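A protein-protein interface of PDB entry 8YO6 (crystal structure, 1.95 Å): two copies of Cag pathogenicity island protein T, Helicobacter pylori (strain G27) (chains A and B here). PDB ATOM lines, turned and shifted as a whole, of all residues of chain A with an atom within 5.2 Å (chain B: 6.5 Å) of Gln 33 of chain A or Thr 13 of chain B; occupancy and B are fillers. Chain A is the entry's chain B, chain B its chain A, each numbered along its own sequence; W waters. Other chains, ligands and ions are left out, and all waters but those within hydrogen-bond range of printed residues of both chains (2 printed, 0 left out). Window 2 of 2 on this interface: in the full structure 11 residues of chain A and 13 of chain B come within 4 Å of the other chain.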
ATOM      1  N   VAL A  19      -7.729 -22.417  20.355  1.00  0.00           N
ATOM      2  CA  VAL A  19      -7.306 -23.814  20.399  1.00  0.00           C
ATOM      3  C   VAL A  19      -7.975 -24.592  19.273  1.00  0.00           C
ATOM      4  O   VAL A  19      -9.140 -24.351  18.934  1.00  0.00           O
ATOM      5  CB  VAL A  19      -7.610 -24.481  21.759  1.00  0.00           C
ATOM      6  CG1 VAL A  19      -6.710 -23.928  22.843  1.00  0.00           C
ATOM      7  CG2 VAL A  19      -9.059 -24.310  22.121  1.00  0.00           C
ATOM      8  N   LYS A  20      -7.239 -25.545  18.714  1.00  0.00           N
ATOM      9  CA  LYS A  20      -7.764 -26.432  17.690  1.00  0.00           C
ATOM     10  C   LYS A  20      -8.230 -27.713  18.371  1.00  0.00           C
ATOM     11  O   LYS A  20      -7.443 -28.372  19.069  1.00  0.00           O
ATOM     12  CB  LYS A  20      -6.714 -26.722  16.616  1.00  0.00           C
ATOM     13  CG  LYS A  20      -6.185 -25.484  15.886  1.00  0.00           C
ATOM     14  CD  LYS A  20      -4.989 -25.868  14.989  1.00  0.00           C
ATOM     15  CE  LYS A  20      -4.538 -24.703  14.119  1.00  0.00           C
ATOM     16  NZ  LYS A  20      -5.488 -23.534  14.187  1.00  0.00           N
ATOM     17  N   LEU A  21      -9.530 -28.045  18.190  1.00  0.00           N
ATOM     18  CA  LEU A  21     -10.179 -29.169  18.831  1.00  0.00           C
ATOM     19  C   LEU A  21     -10.606 -30.186  17.769  1.00  0.00           C
ATOM     20  O   LEU A  21     -10.896 -29.816  16.626  1.00  0.00           O
ATOM     21  CB  LEU A  21     -11.420 -28.729  19.625  1.00  0.00           C
ATOM     22  CG  LEU A  21     -11.168 -27.787  20.813  1.00  0.00           C
ATOM     23  CD1 LEU A  21     -12.492 -27.273  21.412  1.00  0.00           C
ATOM     24  CD2 LEU A  21     -10.203 -28.338  21.863  1.00  0.00           C
ATOM     25  N   PRO A  22     -10.643 -31.466  18.112  1.00  0.00           N
ATOM     26  CA  PRO A  22     -11.046 -32.493  17.143  1.00  0.00           C
ATOM     27  C   PRO A  22     -12.554 -32.634  17.011  1.00  0.00           C
ATOM     28  O   PRO A  22     -13.319 -31.761  17.439  1.00  0.00           O
ATOM     29  CB  PRO A  22     -10.429 -33.765  17.726  1.00  0.00           C
ATOM     30  CG  PRO A  22     -10.480 -33.528  19.197  1.00  0.00           C
ATOM     31  CD  PRO A  22     -10.185 -32.060  19.379  1.00  0.00           C
ATOM     32  N   TYR A  27     -12.801 -35.794  21.045  1.00  0.00           N
ATOM     33  CA  TYR A  27     -12.473 -34.857  22.115  1.00  0.00           C
ATOM     34  C   TYR A  27     -12.804 -35.427  23.487  1.00  0.00           C
ATOM     35  O   TYR A  27     -12.011 -35.301  24.427  1.00  0.00           O
ATOM     36  CB  TYR A  27     -13.219 -33.546  21.868  1.00  0.00           C
ATOM     37  CG  TYR A  27     -13.479 -32.681  23.078  1.00  0.00           C
ATOM     38  CD1 TYR A  27     -12.487 -31.863  23.613  1.00  0.00           C
ATOM     39  CD2 TYR A  27     -14.732 -32.663  23.673  1.00  0.00           C
ATOM     40  CE1 TYR A  27     -12.741 -31.060  24.712  1.00  0.00           C
ATOM     41  CE2 TYR A  27     -14.992 -31.867  24.767  1.00  0.00           C
ATOM     42  CZ  TYR A  27     -14.001 -31.070  25.284  1.00  0.00           C
ATOM     43  OH  TYR A  27     -14.282 -30.284  26.374  1.00  0.00           O
ATOM     44  N   ASP A  30     -10.110 -37.561  24.929  1.00  0.00           N
ATOM     45  CA  ASP A  30      -8.849 -36.902  25.273  1.00  0.00           C
ATOM     46  C   ASP A  30      -9.069 -36.168  26.594  1.00  0.00           C
ATOM     47  O   ASP A  30      -9.498 -35.014  26.621  1.00  0.00           O
ATOM     48  CB  ASP A  30      -8.409 -35.951  24.162  1.00  0.00           C
ATOM     49  CG  ASP A  30      -6.998 -35.418  24.362  1.00  0.00           C
ATOM     50  OD1 ASP A  30      -6.554 -35.259  25.523  1.00  0.00           O
ATOM     51  OD2 ASP A  30      -6.329 -35.138  23.344  1.00  0.00           O
ATOM     52  N   ASN A  31      -8.760 -36.850  27.698  1.00  0.00           N
ATOM     53  CA  ASN A  31      -9.044 -36.305  29.021  1.00  0.00           C
ATOM     54  C   ASN A  31      -8.281 -35.009  29.269  1.00  0.00           C
ATOM     55  O   ASN A  31      -8.825 -34.060  29.845  1.00  0.00           O
ATOM     56  CB  ASN A  31      -8.698 -37.343  30.096  1.00  0.00           C
ATOM     57  CG  ASN A  31      -9.539 -37.186  31.354  1.00  0.00           C
ATOM     58  OD1 ASN A  31      -9.699 -36.080  31.871  1.00  0.00           O
ATOM     59  ND2 ASN A  31     -10.051 -38.294  31.869  1.00  0.00           N
ATOM     60  N   LYS A  32      -7.023 -34.941  28.837  1.00  0.00           N
ATOM     61  CA  LYS A  32      -6.242 -33.733  29.079  1.00  0.00           C
ATOM     62  C   LYS A  32      -6.849 -32.543  28.347  1.00  0.00           C
ATOM     63  O   LYS A  32      -6.933 -31.440  28.899  1.00  0.00           O
ATOM     64  CB  LYS A  32      -4.789 -33.955  28.657  1.00  0.00           C
ATOM     65  CG  LYS A  32      -3.793 -33.000  29.314  1.00  0.00           C
ATOM     66  CD  LYS A  32      -2.355 -33.522  29.206  1.00  0.00           C
ATOM     67  CE  LYS A  32      -1.603 -32.945  28.010  1.00  0.00           C
ATOM     68  NZ  LYS A  32      -1.514 -31.450  28.041  1.00  0.00           N
ATOM     69  N   GLN A  33      -7.326 -32.767  27.123  1.00  0.00           N
ATOM     70  CA  GLN A  33      -7.934 -31.700  26.334  1.00  0.00           C
ATOM     71  C   GLN A  33      -9.233 -31.216  26.961  1.00  0.00           C
ATOM     72  O   GLN A  33      -9.508 -30.010  26.983  1.00  0.00           O
ATOM     73  CB  GLN A  33      -8.200 -32.211  24.922  1.00  0.00           C
ATOM     74  CG  GLN A  33      -8.512 -31.172  23.869  1.00  0.00           C
ATOM     75  CD  GLN A  33      -8.498 -31.785  22.487  1.00  0.00           C
ATOM     76  OE1 GLN A  33      -9.264 -32.710  22.200  1.00  0.00           O
ATOM     77  NE2 GLN A  33      -7.625 -31.294  21.630  1.00  0.00           N
ATOM     78  N   VAL A  34     -10.038 -32.149  27.477  1.00  0.00           N
ATOM     79  CA  VAL A  34     -11.297 -31.793  28.124  1.00  0.00           C
ATOM     80  C   VAL A  34     -11.048 -30.880  29.320  1.00  0.00           C
ATOM     81  O   VAL A  34     -11.712 -29.849  29.486  1.00  0.00           O
ATOM     82  CB  VAL A  34     -12.062 -33.064  28.533  1.00  0.00           C
ATOM     83  CG1 VAL A  34     -13.243 -32.704  29.429  1.00  0.00           C
ATOM     84  CG2 VAL A  34     -12.506 -33.827  27.295  1.00  0.00           C
ATOM     85  N   VAL A  35     -10.114 -31.264  30.188  1.00  0.00           N
ATOM     86  CA  VAL A  35      -9.799 -30.448  31.358  1.00  0.00           C
ATOM     87  C   VAL A  35      -9.302 -29.070  30.930  1.00  0.00           C
ATOM     88  O   VAL A  35      -9.637 -28.053  31.550  1.00  0.00           O
ATOM     89  CB  VAL A  35      -8.771 -31.172  32.247  1.00  0.00           C
ATOM     90  CG1 VAL A  35      -8.266 -30.245  33.341  1.00  0.00           C
ATOM     91  CG2 VAL A  35      -9.387 -32.424  32.849  1.00  0.00           C
ATOM     92  N   LEU A  36      -8.490 -29.016  29.873  1.00  0.00           N
ATOM     93  CA  LEU A  36      -7.950 -27.735  29.432  1.00  0.00           C
ATOM     94  C   LEU A  36      -9.066 -26.813  28.963  1.00  0.00           C
ATOM     95  O   LEU A  36      -9.101 -25.630  29.322  1.00  0.00           O
ATOM     96  CB  LEU A  36      -6.907 -27.953  28.331  1.00  0.00           C
ATOM     97  CG  LEU A  36      -6.276 -26.785  27.553  1.00  0.00           C
ATOM     98  CD1 LEU A  36      -5.060 -27.323  26.827  1.00  0.00           C
ATOM     99  CD2 LEU A  36      -7.182 -26.098  26.545  1.00  0.00           C
ATOM    100  N   THR A  37      -9.994 -27.340  28.158  1.00  0.00           N
ATOM    101  CA  THR A  37     -11.071 -26.493  27.669  1.00  0.00           C
ATOM    102  C   THR A  37     -11.935 -25.979  28.816  1.00  0.00           C
ATOM    103  O   THR A  37     -12.363 -24.819  28.788  1.00  0.00           O
ATOM    104  CB  THR A  37     -11.927 -27.233  26.622  1.00  0.00           C
ATOM    105  OG1 THR A  37     -12.465 -28.452  27.157  1.00  0.00           O
ATOM    106  CG2 THR A  37     -11.094 -27.558  25.374  1.00  0.00           C
ATOM    107  N   PHE A  38     -12.134 -26.778  29.875  1.00  0.00           N
ATOM    108  CA  PHE A  38     -12.971 -26.282  30.963  1.00  0.00           C
ATOM    109  C   PHE A  38     -12.280 -25.192  31.773  1.00  0.00           C
ATOM    110  O   PHE A  38     -12.947 -24.252  32.221  1.00  0.00           O
ATOM    111  CB  PHE A  38     -13.413 -27.432  31.877  1.00  0.00           C
ATOM    112  CG  PHE A  38     -14.685 -28.076  31.434  1.00  0.00           C
ATOM    113  CD1 PHE A  38     -14.692 -28.940  30.351  1.00  0.00           C
ATOM    114  CD2 PHE A  38     -15.885 -27.765  32.048  1.00  0.00           C
ATOM    115  CE1 PHE A  38     -15.873 -29.527  29.924  1.00  0.00           C
ATOM    116  CE2 PHE A  38     -17.069 -28.348  31.628  1.00  0.00           C
ATOM    117  CZ  PHE A  38     -17.064 -29.228  30.565  1.00  0.00           C
ATOM    118  N   LYS B  11      -0.216 -34.487  20.362  1.00  0.00           N
ATOM    119  CA  LYS B  11      -1.045 -34.923  21.479  1.00  0.00           C
ATOM    120  C   LYS B  11      -1.496 -33.708  22.273  1.00  0.00           C
ATOM    121  O   LYS B  11      -2.653 -33.624  22.690  1.00  0.00           O
ATOM    122  CB  LYS B  11      -0.284 -35.897  22.382  1.00  0.00           C
ATOM    123  CG  LYS B  11       0.187 -37.153  21.676  1.00  0.00           C
ATOM    124  CD  LYS B  11      -0.974 -37.967  21.134  1.00  0.00           C
ATOM    125  CE  LYS B  11      -1.749 -38.627  22.266  1.00  0.00           C
ATOM    126  NZ  LYS B  11      -2.755 -39.598  21.758  1.00  0.00           N
ATOM    127  N   ASP B  12      -0.572 -32.772  22.483  1.00  0.00           N
ATOM    128  CA  ASP B  12      -0.936 -31.500  23.092  1.00  0.00           C
ATOM    129  C   ASP B  12      -1.857 -30.727  22.168  1.00  0.00           C
ATOM    130  O   ASP B  12      -1.695 -30.742  20.945  1.00  0.00           O
ATOM    131  CB  ASP B  12       0.303 -30.666  23.407  1.00  0.00           C
ATOM    132  CG  ASP B  12       1.096 -31.226  24.565  1.00  0.00           C
ATOM    133  OD1 ASP B  12       2.181 -31.804  24.323  1.00  0.00           O
ATOM    134  OD2 ASP B  12       0.633 -31.080  25.720  1.00  0.00           O
ATOM    135  N   THR B  13      -2.822 -30.051  22.761  1.00  0.00           N
ATOM    136  CA  THR B  13      -3.759 -29.249  21.999  1.00  0.00           C
ATOM    137  C   THR B  13      -3.012 -28.098  21.340  1.00  0.00           C
ATOM    138  O   THR B  13      -2.332 -27.336  22.039  1.00  0.00           O
ATOM    139  CB  THR B  13      -4.853 -28.728  22.926  1.00  0.00           C
ATOM    140  OG1 THR B  13      -5.586 -29.834  23.473  1.00  0.00           O
ATOM    141  CG2 THR B  13      -5.796 -27.781  22.186  1.00  0.00           C
ATOM    142  N   PRO B  14      -3.089 -27.932  20.022  1.00  0.00           N
ATOM    143  CA  PRO B  14      -2.488 -26.738  19.409  1.00  0.00           C
ATOM    144  C   PRO B  14      -3.166 -25.484  19.938  1.00  0.00           C
ATOM    145  O   PRO B  14      -4.389 -25.397  19.985  1.00  0.00           O
ATOM    146  CB  PRO B  14      -2.744 -26.934  17.910  1.00  0.00           C
ATOM    147  CG  PRO B  14      -3.029 -28.442  17.753  1.00  0.00           C
ATOM    148  CD  PRO B  14      -3.717 -28.825  19.028  1.00  0.00           C
ATOM    149  N   PHE B  15      -2.369 -24.502  20.339  1.00  0.00           N
ATOM    150  CA  PHE B  15      -2.933 -23.296  20.911  1.00  0.00           C
ATOM    151  C   PHE B  15      -2.196 -22.080  20.377  1.00  0.00           C
ATOM    152  O   PHE B  15      -1.041 -22.157  19.932  1.00  0.00           O
ATOM    153  CB  PHE B  15      -2.883 -23.306  22.449  1.00  0.00           C
ATOM    154  CG  PHE B  15      -1.486 -23.187  23.015  1.00  0.00           C
ATOM    155  CD1 PHE B  15      -0.859 -21.956  23.116  1.00  0.00           C
ATOM    156  CD2 PHE B  15      -0.804 -24.319  23.442  1.00  0.00           C
ATOM    157  CE1 PHE B  15       0.433 -21.846  23.630  1.00  0.00           C
ATOM    158  CE2 PHE B  15       0.490 -24.225  23.964  1.00  0.00           C
ATOM    159  CZ  PHE B  15       1.106 -22.982  24.046  1.00  0.00           C
ATOM    160  N   ASN B  91       2.245 -23.150  20.402  1.00  0.00           N
ATOM    161  CA  ASN B  91       3.026 -24.375  20.378  1.00  0.00           C
ATOM    162  C   ASN B  91       3.138 -24.955  18.979  1.00  0.00           C
ATOM    163  O   ASN B  91       3.473 -26.132  18.827  1.00  0.00           O
ATOM    164  CB  ASN B  91       2.474 -25.417  21.359  1.00  0.00           C
ATOM    165  CG  ASN B  91       1.044 -25.814  21.065  1.00  0.00           C
ATOM    166  OD1 ASN B  91       0.365 -25.201  20.233  1.00  0.00           O
ATOM    167  ND2 ASN B  91       0.588 -26.884  21.725  1.00  0.00           N
ATOM    168  N   TYR B  92       2.860 -24.155  17.959  1.00  0.00           N
ATOM    169  CA  TYR B  92       3.127 -24.539  16.577  1.00  0.00           C
ATOM    170  C   TYR B  92       3.532 -23.293  15.801  1.00  0.00           C
ATOM    171  O   TYR B  92       3.786 -22.239  16.408  1.00  0.00           O
ATOM    172  CB  TYR B  92       1.905 -25.219  15.967  1.00  0.00           C
ATOM    173  CG  TYR B  92       0.681 -24.325  15.893  1.00  0.00           C
ATOM    174  CD1 TYR B  92       0.477 -23.465  14.818  1.00  0.00           C
ATOM    175  CD2 TYR B  92      -0.254 -24.316  16.932  1.00  0.00           C
ATOM    176  CE1 TYR B  92      -0.650 -22.643  14.762  1.00  0.00           C
ATOM    177  CE2 TYR B  92      -1.372 -23.504  16.895  1.00  0.00           C
ATOM    178  CZ  TYR B  92      -1.572 -22.672  15.807  1.00  0.00           C
ATOM    179  OH  TYR B  92      -2.694 -21.870  15.771  1.00  0.00           O
HETATM  180  O   HOH W   1      -4.735 -22.202  17.334  1.00  0.00           O
HETATM  181  O   HOH W   2      -3.998 -21.011  13.139  1.00  0.00           O
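Thr 13 of chain B touches Val 19 of chain A. Val 19 of chain A touches Pro 14 of chain B (CA to O, 3.3 Å). CG1 of Val 19 of chain A touches CB of Phe 15 of chain B, at 3.9 Å. Thr 13 of chain B touches Lys 20 of chain A (CG2 to O, 3.6 Å). Tyr 92 of chain B touches Lys 20 of chain A.
The backbone carbonyl oxygen (O) of Pro 14 of chain B sits at hydrogen-bond distance from the backbone NH (N) of Lys 20 of chain A, at 3.1 Å. OD2 of Asp 12 of chain B lies within salt-bridge range of NZ of Lys 32 of chain A (3.2 Å). The side-chain hydroxyl (OG1) of Thr 13 of chain B lies within hydrogen-bond range of the side-chain amide nitrogen (NE2) of Gln 33 of chain A, at 3.1 Å.
Printed residues of chain B that touch a printed residue of chain A: Asp 12, Thr 13, Pro 14, Phe 15 and Tyr 92. Hydrophobic or aromatic side chains of chain A that line the printed part of chain B: Val 19. Among the printed residues, Asp or Glu carboxylates within 4 Å of a Lys or Arg side-chain nitrogen of the other chain: Lys 32 of chain A with Asp 12 of chain B (3.2 Å).
No position is printed for both chains.
The backbone carbonyl oxygen (O) of Thr 13 of chain B lies within hydrogen-bond range of the side-chain amide nitrogen (ND2) of Asn 91 of chain B (3.0 Å). The side-chain carboxylate of Asp 30 of chain A sits close to the backbone NH of Lys 32 of chain A (3.4 Å). OD1 of Asp 30 of chain A lies within hydrogen-bond range of N of Gln 33 of chain A. The backbone NH of Phe 15 of chain B lies within hydrogen-bond range of the side-chain amide oxygen of Asn 91 of chain B (2.8 Å). The backbone carbonyl oxygen (O) of Gln 33 of chain A lies close to the side-chain hydroxyl (OG1) of Thr 37 of chain A (3.3 Å).
Gln 33 of chain A touches just one residue of chain B: Thr 13 (3.1 Å). Thr 13 of chain B touches just these residues of chain A: Val 19, Lys 20 and Gln 33. Of the printed residues of chain A, Asp 12 of chain B touches Lys 32. Of the printed residues of chain B, Lys 20 of chain A touches Thr 13 (3.6 Å), Pro 14 (3.1 Å) and Tyr 92 (3.6 Å). Printed residues of chain A within 4 Å of Pro 14 of chain B: Val 19 and Lys 20. The nearest residue of chain B that does not touch Gln 33 of chain A is Pro 14 of chain B (5.3 Å).
Water W1 lies within hydrogen-bond range of OH of Tyr 92 of chain B (2.6 Å) and NZ of Lys 20 of chain A (3.5 Å). Water W2 bridges the side-chain hydroxyl (OH) of Tyr 92 of chain B and the side-chain amino group (NZ) of Lys 20 of chain A.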
